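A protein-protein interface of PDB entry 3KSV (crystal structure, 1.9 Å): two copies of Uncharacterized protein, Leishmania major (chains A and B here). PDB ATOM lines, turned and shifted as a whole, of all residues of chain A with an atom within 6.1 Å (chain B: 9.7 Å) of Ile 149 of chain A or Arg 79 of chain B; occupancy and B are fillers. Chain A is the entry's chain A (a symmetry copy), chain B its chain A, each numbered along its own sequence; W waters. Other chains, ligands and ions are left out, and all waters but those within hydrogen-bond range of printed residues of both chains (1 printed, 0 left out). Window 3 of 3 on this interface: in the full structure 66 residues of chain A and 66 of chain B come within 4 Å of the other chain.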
ATOM      1  N   LEU A  59      -6.781 -14.372 -22.752  1.00  0.00           N
ATOM      2  CA  LEU A  59      -5.826 -13.283 -22.881  1.00  0.00           C
ATOM      3  C   LEU A  59      -6.402 -12.124 -23.672  1.00  0.00           C
ATOM      4  O   LEU A  59      -6.083 -10.959 -23.392  1.00  0.00           O
ATOM      5  CB  LEU A  59      -4.516 -13.776 -23.525  1.00  0.00           C
ATOM      6  CG  LEU A  59      -3.349 -12.787 -23.499  1.00  0.00           C
ATOM      7  CD1 LEU A  59      -2.996 -12.388 -22.075  1.00  0.00           C
ATOM      8  CD2 LEU A  59      -2.105 -13.367 -24.225  1.00  0.00           C
ATOM      9  N   HIS A  60      -7.268 -12.443 -24.631  1.00  0.00           N
ATOM     10  CA  HIS A  60      -7.889 -11.422 -25.483  1.00  0.00           C
ATOM     11  C   HIS A  60      -8.910 -10.567 -24.747  1.00  0.00           C
ATOM     12  O   HIS A  60      -9.365  -9.569 -25.290  1.00  0.00           O
ATOM     13  CB  HIS A  60      -8.498 -12.017 -26.776  1.00  0.00           C
ATOM     14  CG  HIS A  60      -9.594 -13.017 -26.561  1.00  0.00           C
ATOM     15  ND1 HIS A  60     -10.934 -12.672 -26.576  1.00  0.00           N
ATOM     16  CD2 HIS A  60      -9.556 -14.359 -26.382  1.00  0.00           C
ATOM     17  CE1 HIS A  60     -11.669 -13.752 -26.360  1.00  0.00           C
ATOM     18  NE2 HIS A  60     -10.854 -14.790 -26.245  1.00  0.00           N
ATOM     19  N   GLU A  61      -9.257 -10.952 -23.516  1.00  0.00           N
ATOM     20  CA  GLU A  61     -10.182 -10.169 -22.713  1.00  0.00           C
ATOM     21  C   GLU A  61      -9.447  -9.232 -21.762  1.00  0.00           C
ATOM     22  O   GLU A  61     -10.071  -8.417 -21.086  1.00  0.00           O
ATOM     23  CB  GLU A  61     -11.108 -11.102 -21.939  1.00  0.00           C
ATOM     24  CG  GLU A  61     -12.146 -11.796 -22.824  1.00  0.00           C
ATOM     25  CD  GLU A  61     -13.110 -12.677 -22.030  1.00  0.00           C
ATOM     26  OE1 GLU A  61     -12.625 -13.653 -21.412  1.00  0.00           O
ATOM     27  OE2 GLU A  61     -14.342 -12.400 -22.027  1.00  0.00           O
ATOM     28  N   LEU A  62      -8.119  -9.337 -21.732  1.00  0.00           N
ATOM     29  CA  LEU A  62      -7.296  -8.577 -20.794  1.00  0.00           C
ATOM     30  C   LEU A  62      -7.135  -7.133 -21.291  1.00  0.00           C
ATOM     31  O   LEU A  62      -6.972  -6.912 -22.494  1.00  0.00           O
ATOM     32  CB  LEU A  62      -5.920  -9.258 -20.680  1.00  0.00           C
ATOM     33  CG  LEU A  62      -5.031  -9.006 -19.465  1.00  0.00           C
ATOM     34  CD1 LEU A  62      -5.763  -9.324 -18.172  1.00  0.00           C
ATOM     35  CD2 LEU A  62      -3.756  -9.815 -19.600  1.00  0.00           C
ATOM     36  N   GLY A  63      -7.183  -6.159 -20.384  1.00  0.00           N
ATOM     37  CA  GLY A  63      -6.967  -4.758 -20.747  1.00  0.00           C
ATOM     38  C   GLY A  63      -5.531  -4.478 -21.165  1.00  0.00           C
ATOM     39  O   GLY A  63      -4.615  -5.157 -20.733  1.00  0.00           O
ATOM     40  N   MET A  64      -5.335  -3.476 -22.011  1.00  0.00           N
ATOM     41  CA  MET A  64      -4.002  -3.142 -22.515  1.00  0.00           C
ATOM     42  C   MET A  64      -3.033  -2.724 -21.393  1.00  0.00           C
ATOM     43  O   MET A  64      -1.881  -3.126 -21.392  1.00  0.00           O
ATOM     44  CB  MET A  64      -4.095  -2.059 -23.609  1.00  0.00           C
ATOM     45  CG  MET A  64      -3.933  -2.535 -25.085  1.00  0.00           C
ATOM     46  SD  MET A  64      -4.208  -4.290 -25.496  1.00  0.00           S
ATOM     47  N   GLU A 144      -5.356  -6.067 -39.593  1.00  0.00           N
ATOM     48  CA  GLU A 144      -6.517  -5.186 -39.516  1.00  0.00           C
ATOM     49  C   GLU A 144      -7.195  -5.279 -38.141  1.00  0.00           C
ATOM     50  O   GLU A 144      -7.592  -4.246 -37.589  1.00  0.00           O
ATOM     51  CB  GLU A 144      -7.511  -5.486 -40.643  1.00  0.00           C
ATOM     52  CG  GLU A 144      -7.001  -5.017 -42.030  1.00  0.00           C
ATOM     53  CD  GLU A 144      -7.959  -5.323 -43.193  1.00  0.00           C
ATOM     54  OE1 GLU A 144      -9.085  -5.834 -42.938  1.00  0.00           O
ATOM     55  OE2 GLU A 144      -7.575  -5.047 -44.365  1.00  0.00           O
ATOM     56  N   ALA A 145      -7.320  -6.492 -37.593  1.00  0.00           N
ATOM     57  CA  ALA A 145      -7.873  -6.677 -36.240  1.00  0.00           C
ATOM     58  C   ALA A 145      -7.034  -5.967 -35.202  1.00  0.00           C
ATOM     59  O   ALA A 145      -7.563  -5.340 -34.305  1.00  0.00           O
ATOM     60  CB  ALA A 145      -7.970  -8.131 -35.891  1.00  0.00           C
ATOM     61  N   ILE A 146      -5.721  -6.069 -35.323  1.00  0.00           N
ATOM     62  CA  ILE A 146      -4.814  -5.434 -34.378  1.00  0.00           C
ATOM     63  C   ILE A 146      -4.799  -3.921 -34.565  1.00  0.00           C
ATOM     64  O   ILE A 146      -4.760  -3.180 -33.576  1.00  0.00           O
ATOM     65  CB  ILE A 146      -3.381  -6.021 -34.477  1.00  0.00           C
ATOM     66  CG1 ILE A 146      -3.376  -7.491 -34.032  1.00  0.00           C
ATOM     67  CG2 ILE A 146      -2.391  -5.204 -33.663  1.00  0.00           C
ATOM     68  CD1 ILE A 146      -2.180  -8.305 -34.548  1.00  0.00           C
ATOM     69  N   ALA A 147      -4.851  -3.460 -35.811  1.00  0.00           N
ATOM     70  CA  ALA A 147      -4.811  -2.026 -36.109  1.00  0.00           C
ATOM     71  C   ALA A 147      -5.936  -1.198 -35.441  1.00  0.00           C
ATOM     72  O   ALA A 147      -5.737  -0.029 -35.096  1.00  0.00           O
ATOM     73  CB  ALA A 147      -4.834  -1.810 -37.627  1.00  0.00           C
ATOM     74  N   LYS A 148      -7.102  -1.811 -35.251  1.00  0.00           N
ATOM     75  CA  LYS A 148      -8.272  -1.116 -34.682  1.00  0.00           C
ATOM     76  C   LYS A 148      -8.472  -1.263 -33.158  1.00  0.00           C
ATOM     77  O   LYS A 148      -9.503  -0.854 -32.633  1.00  0.00           O
ATOM     78  CB  LYS A 148      -9.553  -1.535 -35.424  1.00  0.00           C
ATOM     79  CG  LYS A 148      -9.969  -3.013 -35.272  1.00  0.00           C
ATOM     80  CD  LYS A 148     -11.165  -3.344 -36.201  1.00  0.00           C
ATOM     81  CE  LYS A 148     -11.453  -4.846 -36.266  1.00  0.00           C
ATOM     82  NZ  LYS A 148     -11.668  -5.445 -34.912  1.00  0.00           N
ATOM     83  N   ILE A 149      -7.493  -1.832 -32.455  1.00  0.00           N
ATOM     84  CA  ILE A 149      -7.488  -1.853 -30.978  1.00  0.00           C
ATOM     85  C   ILE A 149      -6.874  -0.551 -30.446  1.00  0.00           C
ATOM     86  O   ILE A 149      -7.530   0.223 -29.741  1.00  0.00           O
ATOM     87  CB  ILE A 149      -6.666  -3.035 -30.436  1.00  0.00           C
ATOM     88  CG1 ILE A 149      -7.213  -4.363 -30.945  1.00  0.00           C
ATOM     89  CG2 ILE A 149      -6.662  -3.048 -28.925  1.00  0.00           C
ATOM     90  CD1 ILE A 149      -6.299  -5.517 -30.591  1.00  0.00           C
ATOM     91  N   VAL B  28       2.606  -8.550 -39.538  1.00  0.00           N
ATOM     92  CA  VAL B  28       1.213  -8.511 -39.016  1.00  0.00           C
ATOM     93  C   VAL B  28       0.974  -7.291 -38.090  1.00  0.00           C
ATOM     94  O   VAL B  28      -0.140  -6.751 -37.993  1.00  0.00           O
ATOM     95  CB  VAL B  28       0.861  -9.861 -38.305  1.00  0.00           C
ATOM     96  CG1 VAL B  28      -0.369  -9.747 -37.420  1.00  0.00           C
ATOM     97  CG2 VAL B  28       0.687 -10.967 -39.349  1.00  0.00           C
ATOM     98  N   ALA B  29       2.030  -6.848 -37.423  1.00  0.00           N
ATOM     99  CA  ALA B  29       1.989  -5.653 -36.596  1.00  0.00           C
ATOM    100  C   ALA B  29       3.424  -5.284 -36.241  1.00  0.00           C
ATOM    101  O   ALA B  29       4.328  -6.126 -36.306  1.00  0.00           O
ATOM    102  CB  ALA B  29       1.169  -5.889 -35.349  1.00  0.00           C
ATOM    103  N   MET B  48       0.833 -17.779 -35.206  1.00  0.00           N
ATOM    104  CA  MET B  48       1.623 -16.586 -35.366  1.00  0.00           C
ATOM    105  C   MET B  48       2.635 -16.459 -34.269  1.00  0.00           C
ATOM    106  O   MET B  48       2.618 -17.218 -33.302  1.00  0.00           O
ATOM    107  CB  MET B  48       0.722 -15.338 -35.444  1.00  0.00           C
ATOM    108  CG  MET B  48      -0.080 -14.973 -34.200  1.00  0.00           C
ATOM    109  SD  MET B  48      -0.883 -13.374 -34.442  1.00  0.00           S
ATOM    110  CE  MET B  48       0.607 -12.344 -34.544  1.00  0.00           C
ATOM    111  N   VAL B  50       5.057 -13.473 -31.942  1.00  0.00           N
ATOM    112  CA  VAL B  50       5.310 -12.111 -31.468  1.00  0.00           C
ATOM    113  C   VAL B  50       6.720 -12.087 -30.889  1.00  0.00           C
ATOM    114  O   VAL B  50       7.025 -12.838 -29.962  1.00  0.00           O
ATOM    115  CB  VAL B  50       4.315 -11.688 -30.360  1.00  0.00           C
ATOM    116  CG1 VAL B  50       4.731 -10.366 -29.729  1.00  0.00           C
ATOM    117  CG2 VAL B  50       2.903 -11.607 -30.910  1.00  0.00           C
ATOM    118  N   GLY B  71       4.216  -7.588 -23.979  1.00  0.00           N
ATOM    119  CA  GLY B  71       2.967  -8.006 -23.323  1.00  0.00           C
ATOM    120  C   GLY B  71       1.728  -7.407 -23.991  1.00  0.00           C
ATOM    121  O   GLY B  71       0.714  -8.089 -24.177  1.00  0.00           O
ATOM    122  N   VAL B  72       1.807  -6.126 -24.334  1.00  0.00           N
ATOM    123  CA  VAL B  72       0.720  -5.423 -24.993  1.00  0.00           C
ATOM    124  C   VAL B  72       0.480  -5.972 -26.401  1.00  0.00           C
ATOM    125  O   VAL B  72      -0.659  -6.255 -26.748  1.00  0.00           O
ATOM    126  CB  VAL B  72       0.984  -3.893 -25.060  1.00  0.00           C
ATOM    127  CG1 VAL B  72       0.100  -3.232 -26.104  1.00  0.00           C
ATOM    128  CG2 VAL B  72       0.766  -3.267 -23.688  1.00  0.00           C
ATOM    129  N   LEU B  73       1.546  -6.136 -27.197  1.00  0.00           N
ATOM    130  CA  LEU B  73       1.396  -6.732 -28.522  1.00  0.00           C
ATOM    131  C   LEU B  73       0.880  -8.166 -28.467  1.00  0.00           C
ATOM    132  O   LEU B  73       0.104  -8.571 -29.328  1.00  0.00           O
ATOM    133  CB  LEU B  73       2.703  -6.694 -29.306  1.00  0.00           C
ATOM    134  CG  LEU B  73       2.582  -7.098 -30.784  1.00  0.00           C
ATOM    135  CD1 LEU B  73       1.365  -6.479 -31.479  1.00  0.00           C
ATOM    136  CD2 LEU B  73       3.901  -6.765 -31.542  1.00  0.00           C
ATOM    137  N   LEU B  74       1.309  -8.931 -27.474  1.00  0.00           N
ATOM    138  CA  LEU B  74       0.811 -10.308 -27.287  1.00  0.00           C
ATOM    139  C   LEU B  74      -0.714 -10.351 -27.053  1.00  0.00           C
ATOM    140  O   LEU B  74      -1.437 -11.162 -27.651  1.00  0.00           O
ATOM    141  CB  LEU B  74       1.535 -10.954 -26.116  1.00  0.00           C
ATOM    142  CG  LEU B  74       1.363 -12.452 -25.892  1.00  0.00           C
ATOM    143  CD1 LEU B  74       1.838 -13.242 -27.111  1.00  0.00           C
ATOM    144  CD2 LEU B  74       2.145 -12.856 -24.629  1.00  0.00           C
ATOM    145  N   ALA B  75      -1.195  -9.453 -26.203  1.00  0.00           N
ATOM    146  CA  ALA B  75      -2.627  -9.330 -25.915  1.00  0.00           C
ATOM    147  C   ALA B  75      -3.406  -8.914 -27.154  1.00  0.00           C
ATOM    148  O   ALA B  75      -4.488  -9.420 -27.403  1.00  0.00           O
ATOM    149  CB  ALA B  75      -2.868  -8.317 -24.764  1.00  0.00           C
ATOM    150  N   LYS B  76      -2.855  -7.982 -27.922  1.00  0.00           N
ATOM    151  CA  LYS B  76      -3.508  -7.536 -29.152  1.00  0.00           C
ATOM    152  C   LYS B  76      -3.581  -8.664 -30.172  1.00  0.00           C
ATOM    153  O   LYS B  76      -4.637  -8.887 -30.782  1.00  0.00           O
ATOM    154  CB  LYS B  76      -2.777  -6.338 -29.758  1.00  0.00           C
ATOM    155  CG  LYS B  76      -2.944  -5.105 -28.941  1.00  0.00           C
ATOM    156  CD  LYS B  76      -2.380  -3.879 -29.604  1.00  0.00           C
ATOM    157  CE  LYS B  76      -2.756  -2.617 -28.819  1.00  0.00           C
ATOM    158  NZ  LYS B  76      -2.247  -1.400 -29.495  1.00  0.00           N
ATOM    159  N   ALA B  77      -2.458  -9.356 -30.347  1.00  0.00           N
ATOM    160  CA  ALA B  77      -2.371 -10.509 -31.226  1.00  0.00           C
ATOM    161  C   ALA B  77      -3.354 -11.613 -30.822  1.00  0.00           C
ATOM    162  O   ALA B  77      -3.993 -12.211 -31.682  1.00  0.00           O
ATOM    163  CB  ALA B  77      -0.910 -11.049 -31.278  1.00  0.00           C
ATOM    164  N   SER B  78      -3.490 -11.885 -29.524  1.00  0.00           N
ATOM    165  CA  SER B  78      -4.496 -12.867 -29.047  1.00  0.00           C
ATOM    166  C   SER B  78      -5.930 -12.495 -29.457  1.00  0.00           C
ATOM    167  O   SER B  78      -6.755 -13.366 -29.719  1.00  0.00           O
ATOM    168  CB  SER B  78      -4.415 -13.036 -27.523  1.00  0.00           C
ATOM    169  OG  SER B  78      -4.939 -11.897 -26.845  1.00  0.00           O
ATOM    170  N   ARG B  79      -6.237 -11.206 -29.513  1.00  0.00           N
ATOM    171  CA  ARG B  79      -7.563 -10.777 -29.941  1.00  0.00           C
ATOM    172  C   ARG B  79      -7.746 -11.083 -31.440  1.00  0.00           C
ATOM    173  O   ARG B  79      -8.833 -11.490 -31.882  1.00  0.00           O
ATOM    174  CB  ARG B  79      -7.754  -9.288 -29.668  1.00  0.00           C
ATOM    175  CG  ARG B  79      -7.828  -8.904 -28.197  1.00  0.00           C
ATOM    176  CD  ARG B  79      -7.534  -7.426 -28.057  1.00  0.00           C
ATOM    177  NE  ARG B  79      -8.174  -6.782 -26.922  1.00  0.00           N
ATOM    178  CZ  ARG B  79      -7.736  -6.830 -25.670  1.00  0.00           C
ATOM    179  NH1 ARG B  79      -6.648  -7.548 -25.319  1.00  0.00           N
ATOM    180  NH2 ARG B  79      -8.409  -6.166 -24.743  1.00  0.00           N
ATOM    181  N   ALA B  80      -6.670 -10.904 -32.216  1.00  0.00           N
ATOM    182  CA  ALA B  80      -6.663 -11.264 -33.641  1.00  0.00           C
ATOM    183  C   ALA B  80      -6.895 -12.758 -33.782  1.00  0.00           C
ATOM    184  O   ALA B  80      -7.749 -13.189 -34.575  1.00  0.00           O
ATOM    185  CB  ALA B  80      -5.348 -10.858 -34.326  1.00  0.00           C
ATOM    186  N   VAL B  81      -6.184 -13.535 -32.977  1.00  0.00           N
ATOM    187  CA  VAL B  81      -6.246 -15.005 -33.059  1.00  0.00           C
ATOM    188  C   VAL B  81      -7.596 -15.546 -32.562  1.00  0.00           C
ATOM    189  O   VAL B  81      -8.093 -16.567 -33.075  1.00  0.00           O
ATOM    190  CB  VAL B  81      -5.037 -15.676 -32.318  1.00  0.00           C
ATOM    191  CG1 VAL B  81      -5.269 -17.160 -32.117  1.00  0.00           C
ATOM    192  CG2 VAL B  81      -3.762 -15.468 -33.093  1.00  0.00           C
ATOM    193  N   ALA B  82      -8.204 -14.854 -31.595  1.00  0.00           N
ATOM    194  CA  ALA B  82      -9.495 -15.290 -31.046  1.00  0.00           C
ATOM    195  C   ALA B  82     -10.605 -15.182 -32.103  1.00  0.00           C
ATOM    196  O   ALA B  82     -11.637 -15.868 -32.006  1.00  0.00           O
ATOM    197  CB  ALA B  82      -9.850 -14.495 -29.773  1.00  0.00           C
ATOM    198  N   GLY B  83     -10.390 -14.343 -33.118  1.00  0.00           N
ATOM    199  CA  GLY B  83     -11.266 -14.300 -34.295  1.00  0.00           C
ATOM    200  C   GLY B  83     -12.362 -13.263 -34.185  1.00  0.00           C
ATOM    201  O   GLY B  83     -12.475 -12.595 -33.167  1.00  0.00           O
ATOM    202  N   PRO B  84     -13.189 -13.121 -35.237  1.00  0.00           N
ATOM    203  CA  PRO B  84     -14.204 -12.075 -35.236  1.00  0.00           C
ATOM    204  C   PRO B  84     -15.208 -12.156 -34.089  1.00  0.00           C
ATOM    205  O   PRO B  84     -15.617 -11.106 -33.592  1.00  0.00           O
ATOM    206  CB  PRO B  84     -14.886 -12.263 -36.589  1.00  0.00           C
ATOM    207  CG  PRO B  84     -13.834 -12.764 -37.435  1.00  0.00           C
ATOM    208  CD  PRO B  84     -13.066 -13.726 -36.569  1.00  0.00           C
ATOM    209  N   ASP B  85     -15.574 -13.372 -33.658  1.00  0.00           N
ATOM    210  CA  ASP B  85     -16.514 -13.545 -32.526  1.00  0.00           C
ATOM    211  C   ASP B  85     -15.854 -14.001 -31.219  1.00  0.00           C
ATOM    212  O   ASP B  85     -16.538 -14.234 -30.225  1.00  0.00           O
ATOM    213  CB  ASP B  85     -17.660 -14.498 -32.903  1.00  0.00           C
ATOM    214  CG  ASP B  85     -17.208 -15.951 -33.029  1.00  0.00           C
ATOM    215  OD1 ASP B  85     -15.969 -16.212 -32.949  1.00  0.00           O
ATOM    216  OD2 ASP B  85     -18.102 -16.826 -33.229  1.00  0.00           O
ATOM    217  N   GLY B  86     -14.527 -14.126 -31.229  1.00  0.00           N
ATOM    218  CA  GLY B  86     -13.761 -14.456 -30.044  1.00  0.00           C
ATOM    219  C   GLY B  86     -13.862 -15.909 -29.621  1.00  0.00           C
ATOM    220  O   GLY B  86     -13.530 -16.232 -28.478  1.00  0.00           O
ATOM    221  N   SER B  87     -14.293 -16.790 -30.525  1.00  0.00           N
ATOM    222  CA  SER B  87     -14.537 -18.195 -30.170  1.00  0.00           C
ATOM    223  C   SER B  87     -13.345 -19.107 -30.392  1.00  0.00           C
ATOM    224  O   SER B  87     -13.419 -20.290 -30.074  1.00  0.00           O
ATOM    225  CB  SER B  87     -15.701 -18.766 -30.979  1.00  0.00           C
ATOM    226  OG  SER B  87     -15.360 -18.874 -32.357  1.00  0.00           O
ATOM    227  N   MET B  88     -12.264 -18.593 -30.976  1.00  0.00           N
ATOM    228  CA  MET B  88     -11.140 -19.460 -31.293  1.00  0.00           C
ATOM    229  C   MET B  88     -10.269 -19.658 -30.068  1.00  0.00           C
ATOM    230  O   MET B  88      -9.818 -18.687 -29.478  1.00  0.00           O
ATOM    231  CB  MET B  88     -10.281 -18.885 -32.405  1.00  0.00           C
ATOM    232  CG  MET B  88      -8.994 -19.682 -32.621  1.00  0.00           C
ATOM    233  SD  MET B  88      -9.253 -21.362 -33.241  1.00  0.00           S
ATOM    234  CE  MET B  88      -9.815 -20.962 -34.911  1.00  0.00           C
ATOM    235  N   TYR B  90      -6.786 -21.113 -28.135  1.00  0.00           N
ATOM    236  CA  TYR B  90      -5.380 -20.998 -28.520  1.00  0.00           C
ATOM    237  C   TYR B  90      -4.417 -21.157 -27.343  1.00  0.00           C
ATOM    238  O   TYR B  90      -4.774 -20.954 -26.185  1.00  0.00           O
ATOM    239  CB  TYR B  90      -5.119 -19.649 -29.227  1.00  0.00           C
ATOM    240  CG  TYR B  90      -5.596 -18.444 -28.414  1.00  0.00           C
ATOM    241  CD1 TYR B  90      -4.720 -17.733 -27.596  1.00  0.00           C
ATOM    242  CD2 TYR B  90      -6.908 -18.016 -28.487  1.00  0.00           C
ATOM    243  CE1 TYR B  90      -5.150 -16.660 -26.866  1.00  0.00           C
ATOM    244  CE2 TYR B  90      -7.352 -16.936 -27.747  1.00  0.00           C
ATOM    245  CZ  TYR B  90      -6.464 -16.269 -26.951  1.00  0.00           C
ATOM    246  OH  TYR B  90      -6.904 -15.217 -26.205  1.00  0.00           O
ATOM    247  N   VAL B  92      -0.554 -19.925 -25.875  1.00  0.00           N
ATOM    248  CA  VAL B  92       0.589 -19.040 -25.946  1.00  0.00           C
ATOM    249  C   VAL B  92       1.778 -19.791 -25.322  1.00  0.00           C
ATOM    250  O   VAL B  92       1.707 -20.277 -24.199  1.00  0.00           O
ATOM    251  CB  VAL B  92       0.339 -17.706 -25.209  1.00  0.00           C
ATOM    252  CG1 VAL B  92       1.615 -16.839 -25.223  1.00  0.00           C
ATOM    253  CG2 VAL B  92      -0.822 -16.948 -25.875  1.00  0.00           C
ATOM    254  N   ILE B 111       1.583 -17.855 -30.748  1.00  0.00           N
ATOM    255  CA  ILE B 111       0.130 -17.879 -30.476  1.00  0.00           C
ATOM    256  C   ILE B 111      -0.492 -18.883 -31.426  1.00  0.00           C
ATOM    257  O   ILE B 111      -0.551 -18.635 -32.631  1.00  0.00           O
ATOM    258  CB  ILE B 111      -0.573 -16.499 -30.587  1.00  0.00           C
ATOM    259  CG1 ILE B 111       0.241 -15.375 -29.904  1.00  0.00           C
ATOM    260  CG2 ILE B 111      -1.991 -16.571 -29.921  1.00  0.00           C
ATOM    261  CD1 ILE B 111       1.511 -14.970 -30.650  1.00  0.00           C
HETATM  262  O   HOH W   1      -3.355  -1.539 -32.354  1.00  0.00           O
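Ile 149 of chain A touches just these residues of chain B: Lys 76 (3.7 Å) and Arg 79 (3.4 Å). Of chain A, only Leu 59 (3.96 Å), His 60 (3.2 Å), Leu 62 (2.8 Å) and Ile 149 (3.4 Å) come within 4 Å of Arg 79 of chain B. No residue of chain B comes within 4 Å of Gly 63 of chain A. Of the printed residues of chain A, Val 28 of chain B touches Ile 146 (3.7 Å). Printed residues of chain B within 4 Å of Leu 59 of chain A: Leu 74 (3.96 Å), Ser 78 (3.5 Å), Arg 79 (3.96 Å) and Tyr 90 (3.6 Å). Printed residues of chain A within 4 Å of Tyr 90 of chain B: Leu 59 (3.6 Å) and His 60 (2.8 Å). Pro 84 of chain B touches none of the printed residues of chain A. The nearest residue of chain B that does not touch Ile 149 of chain A is Ala 75 of chain B (5.4 Å). The nearest residue of chain A that does not touch Arg 79 of chain B is Met 64 of chain A (4.1 Å). The nearest printed residue of chain B that does not touch Met 64 of chain A is Arg 79 of chain B (4.1 Å).
Among the printed residues, merely in contact across the chains: Leu 59 of chain A with Leu 74 of chain B (3.96 Å), Leu 59 of chain A with Ser 78 of chain B (3.5 Å), Leu 59 of chain A with Arg 79 of chain B (3.96 Å), Leu 59 of chain A with Tyr 90 of chain B (3.6 Å), His 60 of chain A with Ala 82 of chain B (3.4 Å), His 60 of chain A with Gly 86 of chain B (3.8 Å), Met 64 of chain A with Val 72 of chain B (3.5 Å), Met 64 of chain A with Lys 76 of chain B (3.8 Å), Ile 146 of chain A with Val 28 of chain B (3.7 Å), Ile 146 of chain A with Ala 29 of chain B (3.998 Å), Ile 146 of chain A with Lys 76 of chain B (3.8 Å), Ile 146 of chain A with Ala 77 of chain B (3.99 Å), Ile 146 of chain A with Ala 80 of chain B (3.9 Å), Ile 149 of chain A with Lys 76 of chain B (3.7 Å) and Ile 149 of chain A with Arg 79 of chain B (3.4 Å).
Water W1 lies within hydrogen-bond range of O of Ile 146 of chain A (2.5 Å) and NZ of Lys 76 of chain B (3.1 Å).
The backbone carbonyl oxygen (O) of Ala 75 of chain B sits at hydrogen-bond distance from the side-chain hydroxyl (OG) of Ser 78 of chain B, 2.6 Å away. The backbone NH of Met 88 of chain B is in hydrogen-bond range of the backbone carbonyl oxygen of Ala 82 of chain B. The backbone NH (N) of Ser 87 of chain B lies within hydrogen-bond range of the backbone carbonyl oxygen (O) of Ala 82 of chain B, at 3.2 Å.
Of the 12 printed residues of chain A, 6 touch a printed residue of chain B. Hydrophobic or aromatic side chains of chain A that line the printed part of chain B: Leu 59, His 60, Met 64, Ile 146 and Ile 149. Along chain A the printed residues that touch a printed residue of chain B span positions 59 to 149. Hydrophobic or aromatic side chains of chain B that line the printed part of chain A: Val 28, Ala 29, Val 72, Leu 74, Ala 80, Ala 82 and Tyr 90. Among the printed residues, 19 pairs touch across the chains.
No position is printed for both chains. Of the 19 pairs that touch across the chains among the printed residues, none has its exchanged pair printed and touching as well.
The side-chain hydroxyl (OH) of Tyr 90 of chain B sits close to the backbone NH (N) of His 60 of chain A (3.2 Å). The guanidinium group (NH1) of Arg 79 of chain B sits close to the backbone carbonyl oxygen (O) of His 60 of chain A (3.4 Å). The backbone NH of His 60 of chain A lies within hydrogen-bond range of the side-chain hydroxyl of Ser 78 of chain B. O of Leu 62 of chain A is in hydrogen-bond range of NH2 of Arg 79 of chain B (2.8 Å).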
